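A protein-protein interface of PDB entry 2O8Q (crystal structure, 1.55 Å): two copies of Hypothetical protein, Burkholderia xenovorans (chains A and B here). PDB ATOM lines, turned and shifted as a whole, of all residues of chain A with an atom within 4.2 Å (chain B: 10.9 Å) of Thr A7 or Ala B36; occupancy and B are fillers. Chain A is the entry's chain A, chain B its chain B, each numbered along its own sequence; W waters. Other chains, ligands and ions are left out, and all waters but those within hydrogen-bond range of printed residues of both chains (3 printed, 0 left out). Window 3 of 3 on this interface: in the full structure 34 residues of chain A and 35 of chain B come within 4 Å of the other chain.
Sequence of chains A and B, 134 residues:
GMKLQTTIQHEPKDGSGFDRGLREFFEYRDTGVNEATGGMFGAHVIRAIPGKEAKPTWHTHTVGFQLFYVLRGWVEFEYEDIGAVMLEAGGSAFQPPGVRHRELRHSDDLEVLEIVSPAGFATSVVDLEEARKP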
ATOM      1  N   LEU A   4      25.885  18.467  12.579  1.00  0.00           N
ATOM      2  CA  LEU A   4      25.675  19.114  13.890  1.00  0.00           C
ATOM      3  C   LEU A   4      26.786  20.135  14.086  1.00  0.00           C
ATOM      4  O   LEU A   4      27.827  20.123  13.411  1.00  0.00           O
ATOM      5  CB  LEU A   4      25.676  18.119  15.034  1.00  0.00           C
ATOM      6  CG  LEU A   4      24.755  16.908  14.852  1.00  0.00           C
ATOM      7  CD1 LEU A   4      24.850  15.955  16.068  1.00  0.00           C
ATOM      8  CD2 LEU A   4      23.298  17.355  14.553  1.00  0.00           C
ATOM      9  N   GLN A   5      26.554  21.037  15.023  1.00  0.00           N
ATOM     10  CA  GLN A   5      27.476  22.118  15.227  1.00  0.00           C
ATOM     11  C   GLN A   5      28.207  21.952  16.550  1.00  0.00           C
ATOM     12  O   GLN A   5      27.623  21.562  17.551  1.00  0.00           O
ATOM     13  CB  GLN A   5      26.707  23.427  15.151  1.00  0.00           C
ATOM     14  CG  GLN A   5      26.120  23.658  13.758  1.00  0.00           C
ATOM     15  N   THR A   6      29.514  22.208  16.548  1.00  0.00           N
ATOM     16  CA  THR A   6      30.298  22.193  17.763  1.00  0.00           C
ATOM     17  C   THR A   6      29.672  23.188  18.729  1.00  0.00           C
ATOM     18  O   THR A   6      29.417  24.329  18.358  1.00  0.00           O
ATOM     19  CB  THR A   6      31.794  22.514  17.524  1.00  0.00           C
ATOM     20  OG1 THR A   6      32.301  21.597  16.545  1.00  0.00           O
ATOM     21  CG2 THR A   6      32.607  22.418  18.795  1.00  0.00           C
ATOM     22  N   THR A   7      29.428  22.742  19.966  1.00  0.00           N
ATOM     23  CA  THR A   7      28.597  23.474  20.905  1.00  0.00           C
ATOM     24  C   THR A   7      29.318  23.617  22.212  1.00  0.00           C
ATOM     25  O   THR A   7      29.619  22.645  22.898  1.00  0.00           O
ATOM     26  CB  THR A   7      27.189  22.828  21.062  1.00  0.00           C
ATOM     27  OG1 THR A   7      26.556  22.842  19.766  1.00  0.00           O
ATOM     28  CG2 THR A   7      26.328  23.614  22.075  1.00  0.00           C
ATOM     29  N   ILE A   8      29.596  24.885  22.534  1.00  0.00           N
ATOM     30  CA  ILE A   8      30.419  25.246  23.687  1.00  0.00           C
ATOM     31  C   ILE A   8      29.554  25.949  24.698  1.00  0.00           C
ATOM     32  O   ILE A   8      28.706  26.780  24.352  1.00  0.00           O
ATOM     33  CB  ILE A   8      31.541  26.229  23.251  1.00  0.00           C
ATOM     34  CG1 ILE A   8      32.355  25.631  22.081  1.00  0.00           C
ATOM     35  CG2 ILE A   8      32.398  26.650  24.455  1.00  0.00           C
ATOM     36  CD1 ILE A   8      33.005  24.248  22.381  1.00  0.00           C
ATOM     37  N   SER A  92      32.265  23.250  28.660  1.00  0.00           N
ATOM     38  CA  SER A  92      31.965  22.001  27.982  1.00  0.00           C
ATOM     39  C   SER A  92      32.038  22.191  26.497  1.00  0.00           C
ATOM     40  O   SER A  92      31.785  23.298  25.982  1.00  0.00           O
ATOM     41  CB  SER A  92      30.579  21.526  28.376  1.00  0.00           C
ATOM     42  OG  SER A  92      29.557  22.464  28.088  1.00  0.00           O
ATOM     43  N   ALA A  93      32.425  21.119  25.802  1.00  0.00           N
ATOM     44  CA  ALA A  93      32.480  21.136  24.368  1.00  0.00           C
ATOM     45  C   ALA A  93      31.854  19.859  23.845  1.00  0.00           C
ATOM     46  O   ALA A  93      32.356  18.755  24.093  1.00  0.00           O
ATOM     47  CB  ALA A  93      33.922  21.236  23.839  1.00  0.00           C
ATOM     48  N   PHE A  94      30.768  20.017  23.100  1.00  0.00           N
ATOM     49  CA  PHE A  94      30.132  18.919  22.377  1.00  0.00           C
ATOM     50  C   PHE A  94      30.760  18.905  20.969  1.00  0.00           C
ATOM     51  O   PHE A  94      30.717  19.918  20.255  1.00  0.00           O
ATOM     52  CB  PHE A  94      28.618  19.113  22.286  1.00  0.00           C
ATOM     53  CG  PHE A  94      27.957  18.212  21.270  1.00  0.00           C
ATOM     54  CD1 PHE A  94      27.784  16.852  21.509  1.00  0.00           C
ATOM     55  CD2 PHE A  94      27.641  18.695  20.032  1.00  0.00           C
ATOM     56  CE1 PHE A  94      27.240  16.041  20.529  1.00  0.00           C
ATOM     57  CE2 PHE A  94      27.111  17.847  19.083  1.00  0.00           C
ATOM     58  CZ  PHE A  94      26.923  16.560  19.354  1.00  0.00           C
ATOM     59  N   ARG B  29      21.833  23.861  34.819  1.00  0.00           N
ATOM     60  CA  ARG B  29      22.595  24.654  33.864  1.00  0.00           C
ATOM     61  C   ARG B  29      22.846  23.750  32.642  1.00  0.00           C
ATOM     62  O   ARG B  29      23.462  22.669  32.754  1.00  0.00           O
ATOM     63  CB  ARG B  29      23.903  25.145  34.445  1.00  0.00           C
ATOM     64  CG  ARG B  29      24.728  25.954  33.485  1.00  0.00           C
ATOM     65  CD  ARG B  29      25.891  26.614  34.159  1.00  0.00           C
ATOM     66  NE  ARG B  29      26.992  25.682  34.470  1.00  0.00           N
ATOM     67  CZ  ARG B  29      27.873  25.229  33.551  1.00  0.00           C
ATOM     68  NH1 ARG B  29      27.764  25.580  32.268  1.00  0.00           N
ATOM     69  NH2 ARG B  29      28.828  24.371  33.924  1.00  0.00           N
ATOM     70  N   ASP B  30      22.358  24.202  31.494  1.00  0.00           N
ATOM     71  CA  ASP B  30      22.411  23.399  30.257  1.00  0.00           C
ATOM     72  C   ASP B  30      23.746  23.569  29.532  1.00  0.00           C
ATOM     73  O   ASP B  30      24.218  24.695  29.343  1.00  0.00           O
ATOM     74  CB  ASP B  30      21.280  23.845  29.337  1.00  0.00           C
ATOM     75  CG  ASP B  30      20.888  22.825  28.294  1.00  0.00           C
ATOM     76  OD1 ASP B  30      21.687  21.981  27.949  1.00  0.00           O
ATOM     77  OD2 ASP B  30      19.753  22.945  27.786  1.00  0.00           O
ATOM     78  N   THR B  31      24.297  22.447  29.039  1.00  0.00           N
ATOM     79  CA  THR B  31      25.494  22.491  28.188  1.00  0.00           C
ATOM     80  C   THR B  31      25.183  22.827  26.743  1.00  0.00           C
ATOM     81  O   THR B  31      26.100  23.122  25.942  1.00  0.00           O
ATOM     82  CB  THR B  31      26.191  21.119  28.134  1.00  0.00           C
ATOM     83  OG1 THR B  31      25.264  20.162  27.590  1.00  0.00           O
ATOM     84  CG2 THR B  31      26.694  20.685  29.556  1.00  0.00           C
ATOM     85  N   GLY B  32      23.904  22.745  26.385  1.00  0.00           N
ATOM     86  CA  GLY B  32      23.509  22.923  25.004  1.00  0.00           C
ATOM     87  C   GLY B  32      23.424  21.662  24.186  1.00  0.00           C
ATOM     88  O   GLY B  32      23.090  21.724  23.006  1.00  0.00           O
ATOM     89  N   VAL B  33      23.716  20.509  24.795  1.00  0.00           N
ATOM     90  CA  VAL B  33      23.735  19.247  24.073  1.00  0.00           C
ATOM     91  C   VAL B  33      22.361  18.885  23.503  1.00  0.00           C
ATOM     92  O   VAL B  33      22.246  18.404  22.388  1.00  0.00           O
ATOM     93  CB  VAL B  33      24.362  18.162  24.960  1.00  0.00           C
ATOM     94  CG1 VAL B  33      24.042  16.735  24.451  1.00  0.00           C
ATOM     95  CG2 VAL B  33      25.900  18.394  25.000  1.00  0.00           C
ATOM     96  N   ASN B  34      21.315  19.123  24.272  1.00  0.00           N
ATOM     97  CA  ASN B  34      19.929  18.828  23.812  1.00  0.00           C
ATOM     98  C   ASN B  34      19.647  19.583  22.512  1.00  0.00           C
ATOM     99  O   ASN B  34      19.328  18.990  21.490  1.00  0.00           O
ATOM    100  CB  ASN B  34      18.944  19.225  24.931  1.00  0.00           C
ATOM    101  CG  ASN B  34      17.496  19.089  24.552  1.00  0.00           C
ATOM    102  OD1 ASN B  34      17.096  18.430  23.576  1.00  0.00           O
ATOM    103  ND2 ASN B  34      16.656  19.700  25.383  1.00  0.00           N
ATOM    104  N   GLU B  35      19.817  20.914  22.517  1.00  0.00           N
ATOM    105  CA  GLU B  35      19.607  21.720  21.306  1.00  0.00           C
ATOM    106  C   GLU B  35      20.528  21.243  20.162  1.00  0.00           C
ATOM    107  O   GLU B  35      20.067  21.097  19.034  1.00  0.00           O
ATOM    108  CB  GLU B  35      19.831  23.204  21.625  1.00  0.00           C
ATOM    109  CG  GLU B  35      19.749  24.089  20.389  1.00  0.00           C
ATOM    110  CD  GLU B  35      19.326  25.470  20.746  1.00  0.00           C
ATOM    111  OE1 GLU B  35      19.856  25.983  21.761  1.00  0.00           O
ATOM    112  OE2 GLU B  35      18.472  26.031  20.020  1.00  0.00           O
ATOM    113  N   ALA B  36      21.788  20.924  20.455  1.00  0.00           N
ATOM    114  CA  ALA B  36      22.749  20.588  19.422  1.00  0.00           C
ATOM    115  C   ALA B  36      22.456  19.281  18.733  1.00  0.00           C
ATOM    116  O   ALA B  36      22.843  19.061  17.579  1.00  0.00           O
ATOM    117  CB  ALA B  36      24.153  20.540  20.005  1.00  0.00           C
ATOM    118  N   THR B  37      21.846  18.383  19.496  1.00  0.00           N
ATOM    119  CA  THR B  37      21.531  17.038  19.024  1.00  0.00           C
ATOM    120  C   THR B  37      20.050  16.795  18.777  1.00  0.00           C
ATOM    121  O   THR B  37      19.658  15.663  18.521  1.00  0.00           O
ATOM    122  CB  THR B  37      22.022  15.945  20.012  1.00  0.00           C
ATOM    123  OG1 THR B  37      21.252  15.981  21.220  1.00  0.00           O
ATOM    124  CG2 THR B  37      23.529  16.085  20.326  1.00  0.00           C
ATOM    125  N   GLY B  38      19.215  17.834  18.751  1.00  0.00           N
ATOM    126  CA  GLY B  38      17.786  17.613  18.539  1.00  0.00           C
ATOM    127  C   GLY B  38      17.114  16.722  19.559  1.00  0.00           C
ATOM    128  O   GLY B  38      16.126  16.057  19.257  1.00  0.00           O
ATOM    129  N   GLY B  39      17.679  16.693  20.754  1.00  0.00           N
ATOM    130  CA  GLY B  39      17.150  15.908  21.842  1.00  0.00           C
ATOM    131  C   GLY B  39      17.611  14.457  21.876  1.00  0.00           C
ATOM    132  O   GLY B  39      17.177  13.675  22.703  1.00  0.00           O
ATOM    133  N   MET B  40      18.514  14.079  20.990  1.00  0.00           N
ATOM    134  CA  MET B  40      19.047  12.715  21.085  1.00  0.00           C
ATOM    135  C   MET B  40      19.815  12.492  22.373  1.00  0.00           C
ATOM    136  O   MET B  40      19.808  11.374  22.902  1.00  0.00           O
ATOM    137  CB  MET B  40      19.957  12.402  19.891  1.00  0.00           C
ATOM    138  CG  MET B  40      19.314  12.509  18.518  1.00  0.00           C
ATOM    139  SD  MET B  40      20.504  11.795  17.063  1.00  0.00           S
ATOM    140  CE  MET B  40      20.434  10.038  17.842  1.00  0.00           C
ATOM    141  N   PHE B  41      20.521  13.532  22.841  1.00  0.00           N
ATOM    142  CA  PHE B  41      21.225  13.492  24.085  1.00  0.00           C
ATOM    143  C   PHE B  41      20.939  14.793  24.826  1.00  0.00           C
ATOM    144  O   PHE B  41      20.574  15.785  24.228  1.00  0.00           O
ATOM    145  CB  PHE B  41      22.758  13.387  23.877  1.00  0.00           C
ATOM    146  CG  PHE B  41      23.206  12.075  23.375  1.00  0.00           C
ATOM    147  CD1 PHE B  41      23.210  11.811  22.039  1.00  0.00           C
ATOM    148  CD2 PHE B  41      23.659  11.121  24.296  1.00  0.00           C
ATOM    149  CE1 PHE B  41      23.632  10.533  21.600  1.00  0.00           C
ATOM    150  CE2 PHE B  41      24.050   9.857  23.831  1.00  0.00           C
ATOM    151  CZ  PHE B  41      24.012   9.621  22.524  1.00  0.00           C
ATOM    152  N   GLY B  42      21.135  14.765  26.134  1.00  0.00           N
ATOM    153  CA  GLY B  42      21.145  15.942  26.984  1.00  0.00           C
ATOM    154  C   GLY B  42      22.307  15.884  27.947  1.00  0.00           C
ATOM    155  O   GLY B  42      22.769  14.790  28.288  1.00  0.00           O
ATOM    156  N   ALA B  43      22.780  17.065  28.361  1.00  0.00           N
ATOM    157  CA  ALA B  43      23.792  17.121  29.394  1.00  0.00           C
ATOM    158  C   ALA B  43      23.654  18.432  30.126  1.00  0.00           C
ATOM    159  O   ALA B  43      23.545  19.483  29.535  1.00  0.00           O
ATOM    160  CB  ALA B  43      25.179  16.933  28.863  1.00  0.00           C
ATOM    161  N   ALA B 119      17.249  13.340  25.720  1.00  0.00           N
ATOM    162  CA  ALA B 119      17.093  14.477  26.608  1.00  0.00           C
ATOM    163  C   ALA B 119      15.727  14.467  27.298  1.00  0.00           C
ATOM    164  O   ALA B 119      15.584  14.827  28.484  1.00  0.00           O
ATOM    165  CB  ALA B 119      17.323  15.782  25.867  1.00  0.00           C
HETATM  166  O   HOH W   1      29.329  24.042  30.484  1.00  0.00           O
HETATM  167  O   HOH W   2      28.633  22.187  25.534  1.00  0.00           O
HETATM  168  O   HOH W   3      23.800  21.182  16.086  1.00  0.00           O
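The side-chain hydroxyl (OG1) of Thr A7 is in hydrogen-bond range of the backbone carbonyl oxygen (O) of Gln A5 (2.8 Å). N of Phe A94 sits at hydrogen-bond distance from O of Thr A7 (2.9 Å). The backbone NH (N) of Gly B32 sits at hydrogen-bond distance from the side-chain carboxylate (OD1) of Asp B30. OG1 of Thr B31 sits at hydrogen-bond distance from O of Ala B43, at 2.7 Å. The side-chain hydroxyl of Thr B37 sits at hydrogen-bond distance from the backbone carbonyl oxygen of Val B33 (2.9 Å). The side-chain hydroxyl (OG1) of Thr B37 sits at hydrogen-bond distance from the backbone NH (N) of Phe B41.
Among the printed residues, pairs that only touch across the chains: Thr A7 with Ala B36, Leu A4 with Ala B36, Phe A94 with Thr B37, Ser A92 with Thr B31, Thr A7 with Gly B32, Thr A7 with Thr B31, Phe A94 with Val B33 and Phe A94 with Ala B36.
Of the printed residues of chain B, Thr A7 touches Thr B31, Gly B32 and Ala B36. Of chain A, only Leu A4 (3.5 Å), Thr A7 (3.3 Å) and Phe A94 (3.9 Å) come within 4 Å of Ala B36. Leu A4 touches one residue of chain B. Ile A8 touches none of the printed residues of chain B. Phe A94 touches three residues of chain B. Printed residues of chain A within 4 Å of Thr B37: Phe A94. Of the printed residues of chain A, Val B33 touches Phe A94. Ala B43 touches none of the printed residues of chain A. The nearest residue of chain B that does not touch Thr A7 is Val B33 (4.9 Å).
Water W2 lies within hydrogen-bond range of OG of Ser A92 (2.7 Å), O of Thr B31 (2.7 Å) and O of Thr A7 (2.9 Å). Water W3 bridges O of Ala B36 and N of Gln A5. Water W1 bridges NH1 of Arg B29 (2.8 Å) and OG of Ser A92 (2.9 Å).
Among the printed residues, 8 pairs touch across the chains.
No position is printed for both chains. Of the 8 pairs that touch across the chains among the printed residues, none has its exchanged pair printed and touching as well.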
